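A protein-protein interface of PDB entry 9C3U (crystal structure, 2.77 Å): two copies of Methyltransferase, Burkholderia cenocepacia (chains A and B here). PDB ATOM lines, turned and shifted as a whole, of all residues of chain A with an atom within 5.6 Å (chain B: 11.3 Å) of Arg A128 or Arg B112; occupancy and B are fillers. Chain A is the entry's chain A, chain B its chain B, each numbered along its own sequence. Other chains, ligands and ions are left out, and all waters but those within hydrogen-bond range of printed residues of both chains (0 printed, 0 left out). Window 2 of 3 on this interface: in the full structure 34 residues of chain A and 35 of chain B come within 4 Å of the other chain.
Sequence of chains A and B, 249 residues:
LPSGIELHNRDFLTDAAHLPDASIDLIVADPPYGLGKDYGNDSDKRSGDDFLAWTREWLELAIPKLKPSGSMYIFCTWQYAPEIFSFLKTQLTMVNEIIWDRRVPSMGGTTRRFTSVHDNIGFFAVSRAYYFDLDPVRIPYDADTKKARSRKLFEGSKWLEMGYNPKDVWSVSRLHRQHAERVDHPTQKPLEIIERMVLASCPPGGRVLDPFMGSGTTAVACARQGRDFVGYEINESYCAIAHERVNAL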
ATOM      1  N   THR A  93      -7.571  -8.856  38.661  1.00  0.00           N
ATOM      2  CA  THR A  93      -6.974  -8.018  37.631  1.00  0.00           C
ATOM      3  C   THR A  93      -7.930  -6.891  37.264  1.00  0.00           C
ATOM      4  O   THR A  93      -9.139  -7.104  37.139  1.00  0.00           O
ATOM      5  CB  THR A  93      -6.616  -8.834  36.383  1.00  0.00           C
ATOM      6  OG1 THR A  93      -6.151  -7.955  35.351  1.00  0.00           O
ATOM      7  CG2 THR A  93      -7.821  -9.615  35.874  1.00  0.00           C
ATOM      8  N   VAL A  95      -9.611  -4.600  34.801  1.00  0.00           N
ATOM      9  CA  VAL A  95      -9.917  -4.473  33.383  1.00  0.00           C
ATOM     10  C   VAL A  95     -10.113  -3.013  32.993  1.00  0.00           C
ATOM     11  O   VAL A  95      -9.684  -2.592  31.917  1.00  0.00           O
ATOM     12  CB  VAL A  95     -11.153  -5.329  33.039  1.00  0.00           C
ATOM     13  CG1 VAL A  95     -11.822  -4.835  31.767  1.00  0.00           C
ATOM     14  CG2 VAL A  95     -10.762  -6.791  32.909  1.00  0.00           C
ATOM     15  N   PHE A 123     -13.336  -1.640  37.605  1.00  0.00           N
ATOM     16  CA  PHE A 123     -13.815  -2.793  36.855  1.00  0.00           C
ATOM     17  C   PHE A 123     -12.724  -3.852  36.898  1.00  0.00           C
ATOM     18  O   PHE A 123     -11.709  -3.733  36.198  1.00  0.00           O
ATOM     19  CB  PHE A 123     -14.152  -2.402  35.418  1.00  0.00           C
ATOM     20  CG  PHE A 123     -14.715  -3.523  34.592  1.00  0.00           C
ATOM     21  CD1 PHE A 123     -15.320  -4.617  35.189  1.00  0.00           C
ATOM     22  CD2 PHE A 123     -14.660  -3.468  33.211  1.00  0.00           C
ATOM     23  CE1 PHE A 123     -15.840  -5.641  34.422  1.00  0.00           C
ATOM     24  CE2 PHE A 123     -15.182  -4.487  32.440  1.00  0.00           C
ATOM     25  CZ  PHE A 123     -15.772  -5.575  33.046  1.00  0.00           C
ATOM     26  N   VAL A 126     -11.884 -11.790  37.810  1.00  0.00           N
ATOM     27  CA  VAL A 126     -11.180 -12.883  38.477  1.00  0.00           C
ATOM     28  C   VAL A 126     -10.017 -13.362  37.618  1.00  0.00           C
ATOM     29  O   VAL A 126      -8.880 -13.488  38.089  1.00  0.00           O
ATOM     30  CB  VAL A 126     -12.151 -14.033  38.800  1.00  0.00           C
ATOM     31  N   SER A 127     -10.341 -13.657  36.356  1.00  0.00           N
ATOM     32  CA  SER A 127      -9.333 -14.214  35.426  1.00  0.00           C
ATOM     33  C   SER A 127      -9.436 -13.528  34.062  1.00  0.00           C
ATOM     34  O   SER A 127     -10.347 -12.700  33.883  1.00  0.00           O
ATOM     35  CB  SER A 127      -9.556 -15.683  35.264  1.00  0.00           C
ATOM     36  OG  SER A 127     -10.836 -15.929  34.700  1.00  0.00           O
ATOM     37  N   ARG A 128      -8.564 -13.908  33.132  1.00  0.00           N
ATOM     38  CA  ARG A 128      -8.538 -13.269  31.796  1.00  0.00           C
ATOM     39  C   ARG A 128      -9.639 -13.864  30.919  1.00  0.00           C
ATOM     40  O   ARG A 128      -9.826 -13.372  29.795  1.00  0.00           O
ATOM     41  CB  ARG A 128      -7.162 -13.496  31.172  1.00  0.00           C
ATOM     42  CG  ARG A 128      -6.048 -13.513  32.207  1.00  0.00           C
ATOM     43  CD  ARG A 128      -5.773 -12.123  32.762  1.00  0.00           C
ATOM     44  NE  ARG A 128      -4.374 -11.960  33.170  1.00  0.00           N
ATOM     45  CZ  ARG A 128      -3.346 -11.959  32.333  1.00  0.00           C
ATOM     46  NH1 ARG A 128      -3.513 -11.585  31.078  1.00  0.00           N
ATOM     47  NH2 ARG A 128      -2.153 -12.330  32.756  1.00  0.00           N
ATOM     48  N   ALA A 129     -10.326 -14.887  31.416  1.00  0.00           N
ATOM     49  CA  ALA A 129     -11.459 -15.467  30.663  1.00  0.00           C
ATOM     50  C   ALA A 129     -12.754 -14.923  31.245  1.00  0.00           C
ATOM     51  O   ALA A 129     -13.773 -15.628  31.218  1.00  0.00           O
ATOM     52  CB  ALA A 129     -11.430 -16.970  30.732  1.00  0.00           C
ATOM     53  N   TYR A 130     -12.696 -13.706  31.772  1.00  0.00           N
ATOM     54  CA  TYR A 130     -13.959 -13.085  32.250  1.00  0.00           C
ATOM     55  C   TYR A 130     -14.918 -12.899  31.084  1.00  0.00           C
ATOM     56  O   TYR A 130     -14.489 -12.839  29.923  1.00  0.00           O
ATOM     57  CB  TYR A 130     -13.679 -11.744  32.930  1.00  0.00           C
ATOM     58  CG  TYR A 130     -13.161 -10.649  32.007  1.00  0.00           C
ATOM     59  CD1 TYR A 130     -11.826 -10.610  31.625  1.00  0.00           C
ATOM     60  CD2 TYR A 130     -14.002  -9.654  31.522  1.00  0.00           C
ATOM     61  CE1 TYR A 130     -11.344  -9.624  30.784  1.00  0.00           C
ATOM     62  CE2 TYR A 130     -13.532  -8.662  30.680  1.00  0.00           C
ATOM     63  CZ  TYR A 130     -12.200  -8.648  30.310  1.00  0.00           C
ATOM     64  OH  TYR A 130     -11.714  -7.678  29.486  1.00  0.00           O
ATOM     65  N   TYR A 131     -16.208 -12.785  31.393  1.00  0.00           N
ATOM     66  CA  TYR A 131     -17.232 -12.588  30.336  1.00  0.00           C
ATOM     67  C   TYR A 131     -17.391 -11.108  30.052  1.00  0.00           C
ATOM     68  O   TYR A 131     -17.599 -10.308  30.986  1.00  0.00           O
ATOM     69  CB  TYR A 131     -18.576 -13.184  30.754  1.00  0.00           C
ATOM     70  CG  TYR A 131     -19.785 -12.710  29.960  1.00  0.00           C
ATOM     71  CD1 TYR A 131     -20.037 -13.175  28.677  1.00  0.00           C
ATOM     72  CD2 TYR A 131     -20.684 -11.807  30.504  1.00  0.00           C
ATOM     73  CE1 TYR A 131     -21.144 -12.752  27.963  1.00  0.00           C
ATOM     74  CE2 TYR A 131     -21.791 -11.371  29.800  1.00  0.00           C
ATOM     75  CZ  TYR A 131     -22.025 -11.849  28.528  1.00  0.00           C
ATOM     76  OH  TYR A 131     -23.125 -11.415  27.851  1.00  0.00           O
ATOM     77  N   PHE A 132     -17.298 -10.747  28.776  1.00  0.00           N
ATOM     78  CA  PHE A 132     -17.553  -9.338  28.394  1.00  0.00           C
ATOM     79  C   PHE A 132     -18.250  -9.330  27.053  1.00  0.00           C
ATOM     80  O   PHE A 132     -17.699  -9.840  26.065  1.00  0.00           O
ATOM     81  CB  PHE A 132     -16.310  -8.443  28.338  1.00  0.00           C
ATOM     82  CG  PHE A 132     -16.663  -6.962  28.294  1.00  0.00           C
ATOM     83  CD1 PHE A 132     -16.919  -6.259  29.461  1.00  0.00           C
ATOM     84  CD2 PHE A 132     -16.767  -6.289  27.085  1.00  0.00           C
ATOM     85  CE1 PHE A 132     -17.250  -4.917  29.417  1.00  0.00           C
ATOM     86  CE2 PHE A 132     -17.099  -4.947  27.046  1.00  0.00           C
ATOM     87  CZ  PHE A 132     -17.339  -4.266  28.212  1.00  0.00           C
ATOM     88  N   TRP B  78      -4.683   4.980  34.292  1.00  0.00           N
ATOM     89  CA  TRP B  78      -5.425   4.251  35.314  1.00  0.00           C
ATOM     90  C   TRP B  78      -4.740   2.949  35.709  1.00  0.00           C
ATOM     91  O   TRP B  78      -4.965   2.455  36.819  1.00  0.00           O
ATOM     92  CB  TRP B  78      -6.839   3.967  34.812  1.00  0.00           C
ATOM     93  CG  TRP B  78      -6.853   3.133  33.576  1.00  0.00           C
ATOM     94  CD1 TRP B  78      -6.757   3.571  32.287  1.00  0.00           C
ATOM     95  CD2 TRP B  78      -6.956   1.707  33.508  1.00  0.00           C
ATOM     96  NE1 TRP B  78      -6.800   2.506  31.420  1.00  0.00           N
ATOM     97  CE2 TRP B  78      -6.923   1.350  32.145  1.00  0.00           C
ATOM     98  CE3 TRP B  78      -7.078   0.699  34.468  1.00  0.00           C
ATOM     99  CZ2 TRP B  78      -7.006   0.027  31.719  1.00  0.00           C
ATOM    100  CZ3 TRP B  78      -7.161  -0.614  34.044  1.00  0.00           C
ATOM    101  CH2 TRP B  78      -7.123  -0.938  32.681  1.00  0.00           C
ATOM    102  N   GLN B  79      -3.866   2.423  34.861  1.00  0.00           N
ATOM    103  CA  GLN B  79      -3.217   1.124  35.148  1.00  0.00           C
ATOM    104  C   GLN B  79      -2.200   1.284  36.277  1.00  0.00           C
ATOM    105  O   GLN B  79      -1.898   0.290  36.944  1.00  0.00           O
ATOM    106  CB  GLN B  79      -2.545   0.638  33.870  1.00  0.00           C
ATOM    107  CG  GLN B  79      -3.419   0.752  32.628  1.00  0.00           C
ATOM    108  CD  GLN B  79      -3.027  -0.221  31.540  1.00  0.00           C
ATOM    109  OE1 GLN B  79      -2.200   0.080  30.674  1.00  0.00           O
ATOM    110  NE2 GLN B  79      -3.616  -1.405  31.580  1.00  0.00           N
ATOM    111  N   SER B 106      -8.964   5.974  22.694  1.00  0.00           N
ATOM    112  CA  SER B 106      -7.830   5.224  22.181  1.00  0.00           C
ATOM    113  C   SER B 106      -8.302   4.178  21.180  1.00  0.00           C
ATOM    114  O   SER B 106      -9.378   3.592  21.329  1.00  0.00           O
ATOM    115  CB  SER B 106      -7.071   4.553  23.325  1.00  0.00           C
ATOM    116  OG  SER B 106      -6.126   5.439  23.897  1.00  0.00           O
ATOM    117  N   GLY B 108      -7.460   0.665  18.597  1.00  0.00           N
ATOM    118  CA  GLY B 108      -6.827  -0.634  18.700  1.00  0.00           C
ATOM    119  C   GLY B 108      -7.674  -1.731  18.088  1.00  0.00           C
ATOM    120  O   GLY B 108      -7.196  -2.496  17.247  1.00  0.00           O
ATOM    121  N   GLY B 109      -8.935  -1.813  18.503  1.00  0.00           N
ATOM    122  CA  GLY B 109      -9.852  -2.782  17.935  1.00  0.00           C
ATOM    123  C   GLY B 109     -10.439  -3.736  18.952  1.00  0.00           C
ATOM    124  O   GLY B 109     -11.007  -4.769  18.587  1.00  0.00           O
ATOM    125  N   THR B 110     -10.317  -3.400  20.233  1.00  0.00           N
ATOM    126  CA  THR B 110     -10.774  -4.298  21.279  1.00  0.00           C
ATOM    127  C   THR B 110     -12.296  -4.296  21.379  1.00  0.00           C
ATOM    128  O   THR B 110     -12.985  -3.387  20.908  1.00  0.00           O
ATOM    129  CB  THR B 110     -10.177  -3.911  22.632  1.00  0.00           C
ATOM    130  OG1 THR B 110     -10.769  -4.710  23.663  1.00  0.00           O
ATOM    131  CG2 THR B 110     -10.437  -2.442  22.927  1.00  0.00           C
ATOM    132  N   THR B 111     -12.846  -5.347  21.971  1.00  0.00           N
ATOM    133  CA  THR B 111     -14.306  -5.405  22.179  1.00  0.00           C
ATOM    134  C   THR B 111     -14.515  -6.045  23.530  1.00  0.00           C
ATOM    135  O   THR B 111     -15.678  -6.261  23.913  1.00  0.00           O
ATOM    136  CB  THR B 111     -14.976  -6.178  21.042  1.00  0.00           C
ATOM    137  OG1 THR B 111     -14.358  -5.786  19.821  1.00  0.00           O
ATOM    138  CG2 THR B 111     -16.458  -5.882  20.918  1.00  0.00           C
ATOM    139  N   ARG B 112     -13.416  -6.305  24.244  1.00  0.00           N
ATOM    140  CA  ARG B 112     -13.480  -7.000  25.550  1.00  0.00           C
ATOM    141  C   ARG B 112     -13.339  -6.004  26.696  1.00  0.00           C
ATOM    142  O   ARG B 112     -13.298  -6.448  27.855  1.00  0.00           O
ATOM    143  CB  ARG B 112     -12.295  -7.951  25.691  1.00  0.00           C
ATOM    144  CG  ARG B 112     -12.283  -9.121  24.719  1.00  0.00           C
ATOM    145  CD  ARG B 112     -11.837 -10.400  25.408  1.00  0.00           C
ATOM    146  NE  ARG B 112     -12.075 -10.354  26.854  1.00  0.00           N
ATOM    147  CZ  ARG B 112     -13.003 -11.051  27.488  1.00  0.00           C
ATOM    148  NH1 ARG B 112     -14.256 -11.019  27.077  1.00  0.00           N
ATOM    149  NH2 ARG B 112     -12.672 -11.782  28.534  1.00  0.00           N
ATOM    150  N   ARG B 113     -13.267  -4.714  26.383  1.00  0.00           N
ATOM    151  CA  ARG B 113     -13.079  -3.694  27.436  1.00  0.00           C
ATOM    152  C   ARG B 113     -13.790  -2.396  27.060  1.00  0.00           C
ATOM    153  O   ARG B 113     -14.419  -2.353  25.995  1.00  0.00           O
ATOM    154  CB  ARG B 113     -11.585  -3.413  27.610  1.00  0.00           C
ATOM    155  N   PHE B 114     -13.675  -1.360  27.891  1.00  0.00           N
ATOM    156  CA  PHE B 114     -14.241  -0.027  27.551  1.00  0.00           C
ATOM    157  C   PHE B 114     -13.099   0.858  27.066  1.00  0.00           C
ATOM    158  O   PHE B 114     -12.155   1.070  27.837  1.00  0.00           O
ATOM    159  CB  PHE B 114     -14.982   0.560  28.755  1.00  0.00           C
ATOM    160  CG  PHE B 114     -16.329  -0.054  29.103  1.00  0.00           C
ATOM    161  CD1 PHE B 114     -17.456   0.219  28.341  1.00  0.00           C
ATOM    162  CD2 PHE B 114     -16.468  -0.881  30.210  1.00  0.00           C
ATOM    163  CE1 PHE B 114     -18.682  -0.334  28.671  1.00  0.00           C
ATOM    164  CE2 PHE B 114     -17.696  -1.428  30.535  1.00  0.00           C
ATOM    165  CZ  PHE B 114     -18.799  -1.155  29.764  1.00  0.00           C
ATOM    166  N   THR B 115     -13.182   1.361  25.834  1.00  0.00           N
ATOM    167  CA  THR B 115     -12.100   2.165  25.225  1.00  0.00           C
ATOM    168  C   THR B 115     -11.711   3.333  26.108  1.00  0.00           C
ATOM    169  O   THR B 115     -12.598   3.901  26.758  1.00  0.00           O
ATOM    170  CB  THR B 115     -12.560   2.605  23.841  1.00  0.00           C
ATOM    171  OG1 THR B 115     -13.807   3.258  24.035  1.00  0.00           O
ATOM    172  CG2 THR B 115     -12.741   1.426  22.905  1.00  0.00           C
ATOM    173  N   SER B 116     -10.428   3.705  26.116  1.00  0.00           N
ATOM    174  CA  SER B 116      -9.936   4.777  27.019  1.00  0.00           C
ATOM    175  C   SER B 116     -10.139   6.168  26.417  1.00  0.00           C
ATOM    176  O   SER B 116      -9.843   6.321  25.231  1.00  0.00           O
ATOM    177  CB  SER B 116      -8.489   4.568  27.355  1.00  0.00           C
ATOM    178  OG  SER B 116      -8.027   5.582  28.235  1.00  0.00           O
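The backbone carbonyl oxygen of Arg A128 sits at hydrogen-bond distance from the guanidinium group of Arg B112 (3.5 Å).
The guanidinium group of Arg B112 sits at hydrogen-bond distance from the backbone carbonyl oxygen of Tyr A130 (2.5 Å).
The backbone NH of Phe A132 lies close to the guanidinium group of Arg B112 (3.5 Å).
N of Val A95 sits at hydrogen-bond distance from O of Phe A123.
N of Arg B112 lies within hydrogen-bond range of OG1 of Thr B110 (3.1 Å).
Among the printed residues, merely in contact across the chains: Val A95 with Trp B78 (3.1 Å), Phe A132 with Thr B111 (3.4 Å), Phe A132 with Arg B113 (3.9 Å) and Phe A132 with Phe B114 (3.7 Å).
Of chain B, only Arg B112 comes within 4 Å of Arg A128.
Of chain A, only Arg A128 (3.5 Å), Tyr A130 (2.5 Å) and Phe A132 (3.4 Å) come within 4 Å of Arg B112.
No residue of chain B comes within 4 Å of Val A126.
No residue of chain B comes within 4 Å of Ala A129.
Tyr A130 touches just one residue of chain B: Arg B112.
Of the printed residues of chain B, Phe A132 touches Thr B111 (3.4 Å), Arg B112 (3.4 Å), Arg B113 (3.9 Å) and Phe B114 (3.7 Å).
Of the printed residues of chain A, Trp B78 touches Val A95.
Printed residues of chain A within 4 Å of Thr B111: Phe A132 (3.4 Å).
Printed residues of chain A within 4 Å of Arg B113: Phe A132 (3.9 Å).
Printed residues of chain A within 4 Å of Phe B114: Phe A132 (3.7 Å).
Thr B115 touches none of the printed residues of chain A.
Thr A93 touches none of the printed residues of chain B.
The nearest residue of chain B that does not touch Arg A128 is Arg B113 (9.9 Å).
Of the 10 printed residues of chain A, 4 touch a printed residue of chain B.
Along chain A the printed residues that touch a printed residue of chain B span positions 95 to 132.
Printed residues of chain B that touch a printed residue of chain A: Trp B78, Thr B111, Arg B112, Arg B113 and Phe B114.
Among the printed residues, 7 pairs touch across the chains.
Among the printed residues, no Asp or Glu carboxylate lies within 4 Å of a Lys or Arg side-chain nitrogen of the other chain.
No position is printed for both chains.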
